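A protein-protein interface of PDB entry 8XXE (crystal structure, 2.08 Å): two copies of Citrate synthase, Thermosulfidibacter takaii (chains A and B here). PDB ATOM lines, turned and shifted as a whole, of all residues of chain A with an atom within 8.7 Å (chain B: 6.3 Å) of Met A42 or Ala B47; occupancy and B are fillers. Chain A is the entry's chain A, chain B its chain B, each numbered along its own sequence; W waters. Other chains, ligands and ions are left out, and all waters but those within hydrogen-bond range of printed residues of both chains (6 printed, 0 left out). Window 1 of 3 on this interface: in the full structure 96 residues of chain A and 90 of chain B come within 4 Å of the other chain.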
ATOM      1  N   MET A  31     -24.105 -31.618 -24.106  1.00  0.00           N
ATOM      2  CA  MET A  31     -22.666 -31.778 -23.971  1.00  0.00           C
ATOM      3  C   MET A  31     -22.176 -30.737 -22.966  1.00  0.00           C
ATOM      4  O   MET A  31     -22.960 -29.919 -22.480  1.00  0.00           O
ATOM      5  CB  MET A  31     -21.936 -31.565 -25.306  1.00  0.00           C
ATOM      6  CG  MET A  31     -22.301 -30.218 -25.987  1.00  0.00           C
ATOM      7  SD  MET A  31     -21.576 -29.957 -27.654  1.00  0.00           S
ATOM      8  CE  MET A  31     -19.820 -30.081 -27.353  1.00  0.00           C
ATOM      9  N   CYS A  33     -19.864 -27.451 -22.233  1.00  0.00           N
ATOM     10  CA  CYS A  33     -19.190 -26.302 -22.791  1.00  0.00           C
ATOM     11  C   CYS A  33     -17.887 -26.082 -22.019  1.00  0.00           C
ATOM     12  O   CYS A  33     -17.876 -26.112 -20.797  1.00  0.00           O
ATOM     13  CB  CYS A  33     -20.145 -25.120 -22.705  1.00  0.00           C
ATOM     14  SG  CYS A  33     -19.487 -23.619 -23.469  1.00  0.00           S
ATOM     15  N   THR A  34     -16.778 -25.910 -22.732  1.00  0.00           N
ATOM     16  CA  THR A  34     -15.454 -25.809 -22.132  1.00  0.00           C
ATOM     17  C   THR A  34     -14.794 -24.474 -22.489  1.00  0.00           C
ATOM     18  O   THR A  34     -15.262 -23.766 -23.388  1.00  0.00           O
ATOM     19  CB  THR A  34     -14.590 -27.001 -22.569  1.00  0.00           C
ATOM     20  OG1 THR A  34     -14.197 -26.840 -23.934  1.00  0.00           O
ATOM     21  CG2 THR A  34     -15.292 -28.338 -22.389  1.00  0.00           C
ATOM     22  N   ILE A  35     -13.724 -24.137 -21.749  1.00  0.00           N
ATOM     23  CA  ILE A  35     -12.851 -23.004 -22.026  1.00  0.00           C
ATOM     24  C   ILE A  35     -12.302 -23.091 -23.447  1.00  0.00           C
ATOM     25  O   ILE A  35     -12.192 -22.077 -24.162  1.00  0.00           O
ATOM     26  CB  ILE A  35     -11.734 -22.929 -20.969  1.00  0.00           C
ATOM     27  CG1 ILE A  35     -12.336 -22.596 -19.604  1.00  0.00           C
ATOM     28  CG2 ILE A  35     -10.627 -21.961 -21.377  1.00  0.00           C
ATOM     29  CD1 ILE A  35     -11.347 -22.252 -18.536  1.00  0.00           C
ATOM     30  N   GLY A  36     -11.947 -24.319 -23.832  1.00  0.00           N
ATOM     31  CA  GLY A  36     -11.405 -24.601 -25.149  1.00  0.00           C
ATOM     32  C   GLY A  36     -12.381 -24.180 -26.251  1.00  0.00           C
ATOM     33  O   GLY A  36     -11.899 -23.675 -27.258  1.00  0.00           O
ATOM     34  N   HIS A  37     -13.708 -24.356 -26.030  1.00  0.00           N
ATOM     35  CA  HIS A  37     -14.737 -23.923 -26.974  1.00  0.00           C
ATOM     36  C   HIS A  37     -14.661 -22.412 -27.217  1.00  0.00           C
ATOM     37  O   HIS A  37     -14.770 -21.947 -28.349  1.00  0.00           O
ATOM     38  CB  HIS A  37     -16.157 -24.291 -26.531  1.00  0.00           C
ATOM     39  CG  HIS A  37     -16.489 -25.737 -26.730  1.00  0.00           C
ATOM     40  ND1 HIS A  37     -17.015 -26.525 -25.727  1.00  0.00           N
ATOM     41  CD2 HIS A  37     -16.319 -26.548 -27.794  1.00  0.00           C
ATOM     42  CE1 HIS A  37     -17.142 -27.779 -26.185  1.00  0.00           C
ATOM     43  NE2 HIS A  37     -16.740 -27.815 -27.450  1.00  0.00           N
ATOM     44  N   ALA A  38     -14.515 -21.650 -26.141  1.00  0.00           N
ATOM     45  CA  ALA A  38     -14.529 -20.198 -26.224  1.00  0.00           C
ATOM     46  C   ALA A  38     -13.290 -19.674 -26.956  1.00  0.00           C
ATOM     47  O   ALA A  38     -13.393 -18.754 -27.747  1.00  0.00           O
ATOM     48  CB  ALA A  38     -14.661 -19.607 -24.835  1.00  0.00           C
ATOM     49  N   TYR A  39     -12.115 -20.254 -26.711  1.00  0.00           N
ATOM     50  CA  TYR A  39     -10.914 -19.872 -27.434  1.00  0.00           C
ATOM     51  C   TYR A  39     -10.683 -20.682 -28.716  1.00  0.00           C
ATOM     52  O   TYR A  39      -9.668 -20.489 -29.380  1.00  0.00           O
ATOM     53  CB  TYR A  39      -9.677 -20.107 -26.570  1.00  0.00           C
ATOM     54  CG  TYR A  39      -9.530 -19.145 -25.431  1.00  0.00           C
ATOM     55  CD1 TYR A  39     -10.189 -19.354 -24.230  1.00  0.00           C
ATOM     56  CD2 TYR A  39      -8.785 -17.985 -25.582  1.00  0.00           C
ATOM     57  CE1 TYR A  39     -10.046 -18.466 -23.174  1.00  0.00           C
ATOM     58  CE2 TYR A  39      -8.667 -17.069 -24.554  1.00  0.00           C
ATOM     59  CZ  TYR A  39      -9.275 -17.333 -23.334  1.00  0.00           C
ATOM     60  OH  TYR A  39      -9.165 -16.436 -22.323  1.00  0.00           O
ATOM     61  N   GLY A  40     -11.553 -21.646 -29.031  1.00  0.00           N
ATOM     62  CA  GLY A  40     -11.267 -22.550 -30.120  1.00  0.00           C
ATOM     63  C   GLY A  40     -12.316 -22.401 -31.203  1.00  0.00           C
ATOM     64  O   GLY A  40     -12.520 -23.310 -31.965  1.00  0.00           O
ATOM     65  N   GLY A  41     -13.024 -21.275 -31.207  1.00  0.00           N
ATOM     66  CA  GLY A  41     -14.016 -21.003 -32.222  1.00  0.00           C
ATOM     67  C   GLY A  41     -15.217 -21.937 -32.175  1.00  0.00           C
ATOM     68  O   GLY A  41     -15.799 -22.228 -33.223  1.00  0.00           O
ATOM     69  N   MET A  42     -15.590 -22.376 -30.958  1.00  0.00           N
ATOM     70  CA  MET A  42     -16.803 -23.140 -30.720  1.00  0.00           C
ATOM     71  C   MET A  42     -16.812 -24.481 -31.433  1.00  0.00           C
ATOM     72  O   MET A  42     -17.888 -25.057 -31.593  1.00  0.00           O
ATOM     73  CB  MET A  42     -18.060 -22.410 -31.211  1.00  0.00           C
ATOM     74  CG  MET A  42     -18.307 -21.052 -30.593  1.00  0.00           C
ATOM     75  SD  MET A  42     -19.971 -20.429 -31.067  1.00  0.00           S
ATOM     76  CE  MET A  42     -19.799 -18.686 -30.679  1.00  0.00           C
ATOM     77  N   ARG A  43     -15.660 -24.994 -31.835  1.00  0.00           N
ATOM     78  CA  ARG A  43     -15.581 -26.256 -32.559  1.00  0.00           C
ATOM     79  C   ARG A  43     -16.302 -27.358 -31.798  1.00  0.00           C
ATOM     80  O   ARG A  43     -15.977 -27.600 -30.648  1.00  0.00           O
ATOM     81  CB  ARG A  43     -14.129 -26.697 -32.767  1.00  0.00           C
ATOM     82  CG  ARG A  43     -13.929 -27.607 -33.972  1.00  0.00           C
ATOM     83  CD  ARG A  43     -14.242 -26.886 -35.285  1.00  0.00           C
ATOM     84  NE  ARG A  43     -14.035 -25.439 -35.159  1.00  0.00           N
ATOM     85  CZ  ARG A  43     -13.015 -24.756 -35.676  1.00  0.00           C
ATOM     86  NH1 ARG A  43     -12.413 -25.214 -36.757  1.00  0.00           N
ATOM     87  NH2 ARG A  43     -12.641 -23.601 -35.132  1.00  0.00           N
ATOM     88  N   GLY A  44     -17.312 -27.963 -32.441  1.00  0.00           N
ATOM     89  CA  GLY A  44     -18.035 -29.108 -31.898  1.00  0.00           C
ATOM     90  C   GLY A  44     -19.205 -28.703 -31.011  1.00  0.00           C
ATOM     91  O   GLY A  44     -20.035 -29.527 -30.638  1.00  0.00           O
ATOM     92  N   LEU A  45     -19.286 -27.412 -30.677  1.00  0.00           N
ATOM     93  CA  LEU A  45     -20.303 -26.985 -29.743  1.00  0.00           C
ATOM     94  C   LEU A  45     -21.655 -26.934 -30.451  1.00  0.00           C
ATOM     95  O   LEU A  45     -21.782 -26.291 -31.498  1.00  0.00           O
ATOM     96  CB  LEU A  45     -19.874 -25.633 -29.183  1.00  0.00           C
ATOM     97  CG  LEU A  45     -20.610 -25.181 -27.932  1.00  0.00           C
ATOM     98  CD1 LEU A  45     -20.243 -26.061 -26.726  1.00  0.00           C
ATOM     99  CD2 LEU A  45     -20.287 -23.719 -27.669  1.00  0.00           C
ATOM    100  N   LYS A  46     -22.650 -27.650 -29.892  1.00  0.00           N
ATOM    101  CA  LYS A  46     -23.994 -27.776 -30.466  1.00  0.00           C
ATOM    102  C   LYS A  46     -24.858 -26.557 -30.120  1.00  0.00           C
ATOM    103  O   LYS A  46     -25.742 -26.610 -29.262  1.00  0.00           O
ATOM    104  CB  LYS A  46     -24.632 -29.090 -29.992  1.00  0.00           C
ATOM    105  CG  LYS A  46     -23.985 -30.365 -30.528  1.00  0.00           C
ATOM    106  CD  LYS A  46     -24.632 -31.617 -29.968  1.00  0.00           C
ATOM    107  CE  LYS A  46     -24.211 -32.886 -30.672  1.00  0.00           C
ATOM    108  NZ  LYS A  46     -22.782 -33.174 -30.440  1.00  0.00           N
ATOM    109  N   ALA A  47     -24.633 -25.442 -30.839  1.00  0.00           N
ATOM    110  CA  ALA A  47     -25.049 -24.119 -30.400  1.00  0.00           C
ATOM    111  C   ALA A  47     -26.152 -23.520 -31.276  1.00  0.00           C
ATOM    112  O   ALA A  47     -26.702 -22.467 -30.921  1.00  0.00           O
ATOM    113  CB  ALA A  47     -23.843 -23.201 -30.355  1.00  0.00           C
ATOM    114  N   LEU A  48     -26.498 -24.214 -32.370  1.00  0.00           N
ATOM    115  CA  LEU A  48     -27.325 -23.674 -33.443  1.00  0.00           C
ATOM    116  C   LEU A  48     -28.261 -24.769 -33.909  1.00  0.00           C
ATOM    117  O   LEU A  48     -27.865 -25.929 -33.838  1.00  0.00           O
ATOM    118  CB  LEU A  48     -26.454 -23.313 -34.661  1.00  0.00           C
ATOM    119  CG  LEU A  48     -25.573 -22.082 -34.536  1.00  0.00           C
ATOM    120  CD1 LEU A  48     -25.022 -21.702 -35.892  1.00  0.00           C
ATOM    121  CD2 LEU A  48     -26.359 -20.927 -33.958  1.00  0.00           C
ATOM    122  N   GLY A 241     -23.468 -24.043 -39.336  1.00  0.00           N
ATOM    123  CA  GLY A 241     -22.326 -23.623 -38.526  1.00  0.00           C
ATOM    124  C   GLY A 241     -21.152 -22.987 -39.286  1.00  0.00           C
ATOM    125  O   GLY A 241     -20.253 -22.393 -38.676  1.00  0.00           O
ATOM    126  N   HIS A 246     -23.831 -19.054 -40.704  1.00  0.00           N
ATOM    127  CA  HIS A 246     -23.957 -18.627 -39.330  1.00  0.00           C
ATOM    128  C   HIS A 246     -24.085 -17.108 -39.282  1.00  0.00           C
ATOM    129  O   HIS A 246     -24.895 -16.562 -38.534  1.00  0.00           O
ATOM    130  CB  HIS A 246     -22.728 -19.114 -38.568  1.00  0.00           C
ATOM    131  CG  HIS A 246     -22.767 -18.785 -37.104  1.00  0.00           C
ATOM    132  ND1 HIS A 246     -21.675 -18.894 -36.268  1.00  0.00           N
ATOM    133  CD2 HIS A 246     -23.778 -18.365 -36.341  1.00  0.00           C
ATOM    134  CE1 HIS A 246     -22.025 -18.498 -35.056  1.00  0.00           C
ATOM    135  NE2 HIS A 246     -23.291 -18.177 -35.083  1.00  0.00           N
ATOM    136  N   LEU A 250     -27.200 -15.127 -37.611  1.00  0.00           N
ATOM    137  CA  LEU A 250     -26.943 -14.204 -36.526  1.00  0.00           C
ATOM    138  C   LEU A 250     -27.575 -12.843 -36.813  1.00  0.00           C
ATOM    139  O   LEU A 250     -28.308 -12.273 -35.994  1.00  0.00           O
ATOM    140  CB  LEU A 250     -25.420 -14.166 -36.353  1.00  0.00           C
ATOM    141  CG  LEU A 250     -24.856 -13.074 -35.461  1.00  0.00           C
ATOM    142  CD1 LEU A 250     -25.509 -13.112 -34.088  1.00  0.00           C
ATOM    143  CD2 LEU A 250     -23.350 -13.239 -35.342  1.00  0.00           C
ATOM    144  N   GLU A 420     -29.696 -14.228 -31.357  1.00  0.00           N
ATOM    145  CA  GLU A 420     -28.515 -14.949 -30.949  1.00  0.00           C
ATOM    146  C   GLU A 420     -27.658 -14.028 -30.082  1.00  0.00           C
ATOM    147  O   GLU A 420     -27.273 -12.942 -30.526  1.00  0.00           O
ATOM    148  CB  GLU A 420     -27.790 -15.451 -32.191  1.00  0.00           C
ATOM    149  CG  GLU A 420     -26.552 -16.248 -31.871  1.00  0.00           C
ATOM    150  CD  GLU A 420     -25.845 -16.846 -33.079  1.00  0.00           C
ATOM    151  OE1 GLU A 420     -24.634 -17.040 -32.960  1.00  0.00           O
ATOM    152  OE2 GLU A 420     -26.511 -17.138 -34.120  1.00  0.00           O
ATOM    153  N   ARG A 421     -27.337 -14.479 -28.855  1.00  0.00           N
ATOM    154  CA  ARG A 421     -26.676 -13.647 -27.860  1.00  0.00           C
ATOM    155  C   ARG A 421     -25.901 -14.525 -26.866  1.00  0.00           C
ATOM    156  O   ARG A 421     -26.318 -14.746 -25.751  1.00  0.00           O
ATOM    157  CB  ARG A 421     -27.719 -12.778 -27.151  1.00  0.00           C
ATOM    158  CG  ARG A 421     -27.227 -11.395 -26.750  1.00  0.00           C
ATOM    159  CD  ARG A 421     -28.316 -10.636 -26.004  1.00  0.00           C
ATOM    160  NE  ARG A 421     -28.508 -11.125 -24.637  1.00  0.00           N
ATOM    161  CZ  ARG A 421     -29.324 -10.581 -23.736  1.00  0.00           C
ATOM    162  NH1 ARG A 421     -29.986  -9.479 -24.035  1.00  0.00           N
ATOM    163  NH2 ARG A 421     -29.463 -11.130 -22.535  1.00  0.00           N
ATOM    164  N   PRO A 422     -24.752 -15.097 -27.243  1.00  0.00           N
ATOM    165  CA  PRO A 422     -23.931 -15.848 -26.308  1.00  0.00           C
ATOM    166  C   PRO A 422     -23.235 -14.892 -25.349  1.00  0.00           C
ATOM    167  O   PRO A 422     -23.358 -13.673 -25.453  1.00  0.00           O
ATOM    168  CB  PRO A 422     -22.888 -16.580 -27.170  1.00  0.00           C
ATOM    169  CG  PRO A 422     -22.880 -15.828 -28.519  1.00  0.00           C
ATOM    170  CD  PRO A 422     -24.171 -15.033 -28.594  1.00  0.00           C
ATOM    171  N   LYS A 423     -22.509 -15.490 -24.408  1.00  0.00           N
ATOM    172  CA  LYS A 423     -21.756 -14.782 -23.389  1.00  0.00           C
ATOM    173  C   LYS A 423     -20.288 -14.874 -23.763  1.00  0.00           C
ATOM    174  O   LYS A 423     -19.782 -15.952 -24.077  1.00  0.00           O
ATOM    175  CB  LYS A 423     -22.046 -15.453 -22.041  1.00  0.00           C
ATOM    176  CG  LYS A 423     -21.307 -14.893 -20.841  1.00  0.00           C
ATOM    177  CD  LYS A 423     -21.687 -13.475 -20.503  1.00  0.00           C
ATOM    178  CE  LYS A 423     -20.823 -12.936 -19.378  1.00  0.00           C
ATOM    179  NZ  LYS A 423     -21.076 -11.494 -19.157  1.00  0.00           N
ATOM    180  N   SER A 424     -19.597 -13.733 -23.713  1.00  0.00           N
ATOM    181  CA  SER A 424     -18.160 -13.737 -23.878  1.00  0.00           C
ATOM    182  C   SER A 424     -17.537 -13.894 -22.494  1.00  0.00           C
ATOM    183  O   SER A 424     -18.114 -13.473 -21.507  1.00  0.00           O
ATOM    184  CB  SER A 424     -17.672 -12.486 -24.622  1.00  0.00           C
ATOM    185  OG  SER A 424     -18.128 -11.307 -23.970  1.00  0.00           O
ATOM    186  N   ILE A 425     -16.355 -14.514 -22.428  1.00  0.00           N
ATOM    187  CA  ILE A 425     -15.581 -14.555 -21.192  1.00  0.00           C
ATOM    188  C   ILE A 425     -14.259 -13.831 -21.412  1.00  0.00           C
ATOM    189  O   ILE A 425     -13.773 -13.718 -22.543  1.00  0.00           O
ATOM    190  CB  ILE A 425     -15.325 -16.018 -20.740  1.00  0.00           C
ATOM    191  CG1 ILE A 425     -14.450 -16.772 -21.740  1.00  0.00           C
ATOM    192  CG2 ILE A 425     -16.630 -16.749 -20.480  1.00  0.00           C
ATOM    193  CD1 ILE A 425     -14.252 -18.262 -21.427  1.00  0.00           C
ATOM    194  N   MET B  42     -28.481 -19.264 -27.903  1.00  0.00           N
ATOM    195  CA  MET B  42     -27.228 -19.448 -27.185  1.00  0.00           C
ATOM    196  C   MET B  42     -27.199 -18.615 -25.909  1.00  0.00           C
ATOM    197  O   MET B  42     -26.116 -18.298 -25.410  1.00  0.00           O
ATOM    198  CB  MET B  42     -26.040 -18.951 -28.020  1.00  0.00           C
ATOM    199  CG  MET B  42     -25.721 -19.734 -29.234  1.00  0.00           C
ATOM    200  SD  MET B  42     -24.112 -19.194 -29.877  1.00  0.00           S
ATOM    201  CE  MET B  42     -24.322 -19.642 -31.597  1.00  0.00           C
ATOM    202  N   GLY B  44     -26.575 -17.134 -22.659  1.00  0.00           N
ATOM    203  CA  GLY B  44     -25.817 -17.525 -21.475  1.00  0.00           C
ATOM    204  C   GLY B  44     -24.691 -18.508 -21.779  1.00  0.00           C
ATOM    205  O   GLY B  44     -23.877 -18.782 -20.914  1.00  0.00           O
ATOM    206  N   LEU B  45     -24.601 -19.006 -23.020  1.00  0.00           N
ATOM    207  CA  LEU B  45     -23.585 -19.996 -23.335  1.00  0.00           C
ATOM    208  C   LEU B  45     -22.219 -19.316 -23.470  1.00  0.00           C
ATOM    209  O   LEU B  45     -22.062 -18.370 -24.248  1.00  0.00           O
ATOM    210  CB  LEU B  45     -24.015 -20.746 -24.600  1.00  0.00           C
ATOM    211  CG  LEU B  45     -23.162 -21.953 -24.961  1.00  0.00           C
ATOM    212  CD1 LEU B  45     -23.276 -23.022 -23.879  1.00  0.00           C
ATOM    213  CD2 LEU B  45     -23.586 -22.521 -26.316  1.00  0.00           C
ATOM    214  N   LYS B  46     -21.218 -19.793 -22.713  1.00  0.00           N
ATOM    215  CA  LYS B  46     -19.931 -19.106 -22.644  1.00  0.00           C
ATOM    216  C   LYS B  46     -19.056 -19.502 -23.837  1.00  0.00           C
ATOM    217  O   LYS B  46     -18.143 -20.314 -23.732  1.00  0.00           O
ATOM    218  CB  LYS B  46     -19.267 -19.382 -21.293  1.00  0.00           C
ATOM    219  CG  LYS B  46     -19.998 -18.809 -20.088  1.00  0.00           C
ATOM    220  CD  LYS B  46     -19.085 -18.748 -18.866  1.00  0.00           C
ATOM    221  CE  LYS B  46     -19.732 -19.173 -17.573  1.00  0.00           C
ATOM    222  NZ  LYS B  46     -20.577 -18.116 -16.994  1.00  0.00           N
ATOM    223  N   ALA B  47     -19.337 -18.897 -24.999  1.00  0.00           N
ATOM    224  CA  ALA B  47     -18.901 -19.447 -26.268  1.00  0.00           C
ATOM    225  C   ALA B  47     -17.875 -18.570 -26.999  1.00  0.00           C
ATOM    226  O   ALA B  47     -17.416 -18.971 -28.066  1.00  0.00           O
ATOM    227  CB  ALA B  47     -20.150 -19.678 -27.091  1.00  0.00           C
ATOM    228  N   LEU B  48     -17.516 -17.393 -26.456  1.00  0.00           N
ATOM    229  CA  LEU B  48     -16.653 -16.435 -27.143  1.00  0.00           C
ATOM    230  C   LEU B  48     -15.666 -15.841 -26.144  1.00  0.00           C
ATOM    231  O   LEU B  48     -15.982 -15.777 -24.976  1.00  0.00           O
ATOM    232  CB  LEU B  48     -17.474 -15.259 -27.696  1.00  0.00           C
ATOM    233  CG  LEU B  48     -18.467 -15.538 -28.813  1.00  0.00           C
ATOM    234  CD1 LEU B  48     -19.346 -14.324 -29.029  1.00  0.00           C
ATOM    235  CD2 LEU B  48     -17.749 -15.896 -30.100  1.00  0.00           C
ATOM    236  N   VAL B  49     -14.563 -15.271 -26.653  1.00  0.00           N
ATOM    237  CA  VAL B  49     -13.622 -14.508 -25.847  1.00  0.00           C
ATOM    238  C   VAL B  49     -13.692 -13.022 -26.199  1.00  0.00           C
ATOM    239  O   VAL B  49     -13.687 -12.643 -27.373  1.00  0.00           O
ATOM    240  CB  VAL B  49     -12.188 -15.040 -25.985  1.00  0.00           C
ATOM    241  CG1 VAL B  49     -11.195 -14.201 -25.186  1.00  0.00           C
ATOM    242  CG2 VAL B  49     -12.115 -16.482 -25.521  1.00  0.00           C
ATOM    243  N   HIS B 246     -20.454  -9.706 -32.045  1.00  0.00           N
ATOM    244  CA  HIS B 246     -20.285 -11.096 -32.427  1.00  0.00           C
ATOM    245  C   HIS B 246     -20.153 -11.236 -33.943  1.00  0.00           C
ATOM    246  O   HIS B 246     -19.297 -11.974 -34.408  1.00  0.00           O
ATOM    247  CB  HIS B 246     -21.428 -11.926 -31.840  1.00  0.00           C
ATOM    248  CG  HIS B 246     -21.360 -13.402 -32.087  1.00  0.00           C
ATOM    249  ND1 HIS B 246     -22.467 -14.222 -31.916  1.00  0.00           N
ATOM    250  CD2 HIS B 246     -20.341 -14.187 -32.454  1.00  0.00           C
ATOM    251  CE1 HIS B 246     -22.118 -15.467 -32.232  1.00  0.00           C
ATOM    252  NE2 HIS B 246     -20.812 -15.474 -32.519  1.00  0.00           N
ATOM    253  N   ILE B 419     -10.965 -19.928 -36.796  1.00  0.00           N
ATOM    254  CA  ILE B 419     -12.248 -19.634 -37.409  1.00  0.00           C
ATOM    255  C   ILE B 419     -13.391 -20.068 -36.496  1.00  0.00           C
ATOM    256  O   ILE B 419     -13.374 -21.130 -35.877  1.00  0.00           O
ATOM    257  CB  ILE B 419     -12.336 -20.315 -38.776  1.00  0.00           C
ATOM    258  CG1 ILE B 419     -13.535 -19.784 -39.563  1.00  0.00           C
ATOM    259  CG2 ILE B 419     -12.333 -21.841 -38.656  1.00  0.00           C
ATOM    260  CD1 ILE B 419     -13.503 -20.141 -41.025  1.00  0.00           C
ATOM    261  N   GLU B 420     -14.434 -19.255 -36.409  1.00  0.00           N
ATOM    262  CA  GLU B 420     -15.557 -19.660 -35.586  1.00  0.00           C
ATOM    263  C   GLU B 420     -16.442 -20.626 -36.385  1.00  0.00           C
ATOM    264  O   GLU B 420     -16.866 -20.310 -37.496  1.00  0.00           O
ATOM    265  CB  GLU B 420     -16.224 -18.396 -35.049  1.00  0.00           C
ATOM    266  CG  GLU B 420     -17.471 -18.696 -34.241  1.00  0.00           C
ATOM    267  CD  GLU B 420     -18.193 -17.453 -33.760  1.00  0.00           C
ATOM    268  OE1 GLU B 420     -19.428 -17.528 -33.588  1.00  0.00           O
ATOM    269  OE2 GLU B 420     -17.524 -16.399 -33.600  1.00  0.00           O
ATOM    270  N   ARG B 421     -16.686 -21.841 -35.847  1.00  0.00           N
ATOM    271  CA  ARG B 421     -17.405 -22.885 -36.569  1.00  0.00           C
ATOM    272  C   ARG B 421     -18.091 -23.822 -35.565  1.00  0.00           C
ATOM    273  O   ARG B 421     -17.629 -24.934 -35.294  1.00  0.00           O
ATOM    274  CB  ARG B 421     -16.478 -23.647 -37.529  1.00  0.00           C
ATOM    275  CG  ARG B 421     -17.168 -24.220 -38.771  1.00  0.00           C
ATOM    276  CD  ARG B 421     -17.899 -25.561 -38.680  1.00  0.00           C
ATOM    277  NE  ARG B 421     -18.441 -26.063 -39.959  1.00  0.00           N
ATOM    278  CZ  ARG B 421     -19.677 -26.552 -40.161  1.00  0.00           C
ATOM    279  NH1 ARG B 421     -20.026 -26.993 -41.362  1.00  0.00           N
ATOM    280  NH2 ARG B 421     -20.564 -26.608 -39.176  1.00  0.00           N
ATOM    281  N   PRO B 422     -19.237 -23.394 -35.001  1.00  0.00           N
ATOM    282  CA  PRO B 422     -20.064 -24.286 -34.196  1.00  0.00           C
ATOM    283  C   PRO B 422     -20.723 -25.406 -35.009  1.00  0.00           C
ATOM    284  O   PRO B 422     -20.683 -25.412 -36.235  1.00  0.00           O
ATOM    285  CB  PRO B 422     -21.110 -23.362 -33.572  1.00  0.00           C
ATOM    286  CG  PRO B 422     -21.165 -22.152 -34.490  1.00  0.00           C
ATOM    287  CD  PRO B 422     -19.800 -22.047 -35.142  1.00  0.00           C
ATOM    288  N   LYS B 423     -21.321 -26.357 -34.286  1.00  0.00           N
ATOM    289  CA  LYS B 423     -22.052 -27.477 -34.852  1.00  0.00           C
ATOM    290  C   LYS B 423     -23.545 -27.164 -34.760  1.00  0.00           C
ATOM    291  O   LYS B 423     -24.021 -26.704 -33.723  1.00  0.00           O
ATOM    292  CB  LYS B 423     -21.626 -28.719 -34.057  1.00  0.00           C
ATOM    293  CG  LYS B 423     -22.290 -30.030 -34.448  1.00  0.00           C
ATOM    294  CD  LYS B 423     -21.932 -30.493 -35.839  1.00  0.00           C
ATOM    295  CE  LYS B 423     -22.876 -31.558 -36.360  1.00  0.00           C
ATOM    296  NZ  LYS B 423     -22.510 -31.968 -37.735  1.00  0.00           N
HETATM  297  O   HOH W   1     -15.561 -18.912 -30.155  1.00  0.00           O
HETATM  298  O   HOH W   2     -24.509 -12.625 -30.988  1.00  0.00           O
HETATM  299  O   HOH W   3     -17.991 -27.463 -35.242  1.00  0.00           O
HETATM  300  O   HOH W   4     -16.577 -21.867 -22.065  1.00  0.00           O
HETATM  301  O   HOH W   5     -25.899 -14.471 -23.142  1.00  0.00           O
HETATM  302  O   HOH W   6     -19.592 -19.854 -37.802  1.00  0.00           O
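Met A42 touches Arg B421, and with the chains exchanged Arg A421 touches Met B42. Lys A46 touches Lys B423, and with the chains exchanged Lys A423 touches Lys B46.
Printed residues of chain B within 4 Å of Cys A33: Leu B45 (3.9 Å) and Lys B46 (3.6 Å). Of chain B, only Ala B47 (3.4 Å), Leu B48 (3.5 Å), His B246 (3.8 Å), Glu B420 (3.2 Å), Arg B421 (3.7 Å) and Pro B422 (3.5 Å) come within 4 Å of Met A42. Of the printed residues of chain B, Leu A250 touches His B246. Printed residues of chain A within 4 Å of Ala B47: His A37, Ala A38, Met A42 and Lys A423. The nearest residue of chain B that does not touch Met A42 is Met B42 (4.4 Å).
The backbone carbonyl oxygen (O) of Lys B46 lies within hydrogen-bond range of the side-chain sulfur (SG) of Cys A33 (3.6 Å). The backbone carbonyl oxygen (O) of Gly A41 sits at hydrogen-bond distance from the backbone NH (N) of Arg B421 (2.8 Å). The guanidinium group (NH2) of Arg A43 lies within hydrogen-bond range of the backbone carbonyl oxygen (O) of Ile B419 (2.7 Å). The backbone carbonyl oxygen of Leu A45 sits at hydrogen-bond distance from the backbone NH of Lys B423 (2.8 Å). N of Ala A47 lies within hydrogen-bond range of O of Lys B423 (3.2 Å). N of Lys A423 is in hydrogen-bond range of O of Leu B45 (2.9 Å). O of Lys A423 lies within hydrogen-bond range of N of Ala B47 (3.1 Å). N of Ile A425 lies within hydrogen-bond range of O of Leu B48, 2.9 Å away. The side-chain carboxylate of Glu A420 lies close to the side-chain sulfur of Met B42.
Water W6 lies within hydrogen-bond range of a ring nitrogen (ND1) of His A246, the backbone carbonyl oxygen of Gly A241 and the backbone carbonyl oxygen of Glu B420.
Printed residues of chain B that touch a printed residue of chain A: Met B42, Gly B44, Leu B45, Lys B46, Ala B47, Leu B48, Val B49, His B246, Ile B419, Glu B420, Arg B421, Pro B422 and Lys B423. Hydrophobic or aromatic side chains of chain B that line the printed part of chain A: Met B42, Leu B45, Ala B47, Leu B48, Val B49, His B246, Ile B419 and Pro B422.
The backbone NH of Lys A46 is in hydrogen-bond range of the side-chain sulfur of Met A31, at 3.4 Å. NE2 of His A246 is in hydrogen-bond range of OE1 of Glu A420 (2.8 Å).
Among the printed residues, pairs that only touch across the chains: Glu A420 with His B246 (3.1 Å), His A246 with Glu B420 (3.1 Å), Met A42 with Glu B420 (3.2 Å), Ser A424 with Leu B48 (3.2 Å), Gly A241 with Pro B422 (3.3 Å), Ala A47 with Met B42 (3.4 Å), Leu A48 with Met B42 (3.4 Å), Met A42 with Ala B47 (3.4 Å), Ile A425 with Val B49 (3.4 Å), Pro A422 with Met B42 (3.4 Å), Ala A38 with Val B49 (3.4 Å), Lys A46 with Lys B423 (3.4 Å), Lys A423 with Lys B46 (3.5 Å), Met A42 with Pro B422 (3.5 Å), Gly A41 with Glu B420 (3.5 Å), Met A42 with Leu B48 (3.5 Å), Pro A422 with Leu B45 (3.5 Å), Gly A241 with Arg B421 (3.5 Å), Ile A425 with Lys B46 (3.6 Å), Arg A421 with Met B42 (3.6 Å), Lys A423 with Leu B48 (3.6 Å), Tyr A39 with Val B49 (3.6 Å), Arg A43 with Arg B421 (3.6 Å), Ala A38 with Ala B47 (3.6 Å), Leu A45 with Pro B422 (3.7 Å), Leu A250 with His B246 (3.7 Å), Met A42 with Arg B421 (3.7 Å), Gly A41 with Ile B419 (3.7 Å), Ala A38 with Lys B46 (3.7 Å), His A246 with Pro B422 (3.7 Å), Leu A45 with Leu B45 (3.8 Å), Leu A48 with Lys B423 (3.8 Å), Pro A422 with His B246 (3.8 Å), Met A42 with His B246 (3.8 Å), Gly A44 with Lys B423 (3.9 Å), Cys A33 with Leu B45 (3.9 Å), Pro A422 with Leu B48 (3.9 Å), Arg A421 with Gly B44 (3.9 Å), His A246 with Met B42 (3.9 Å), Ala A38 with Leu B48 (3.96 Å), Lys A423 with Gly B44 (3.96 Å) and His A37 with Ala B47 (3.99 Å).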
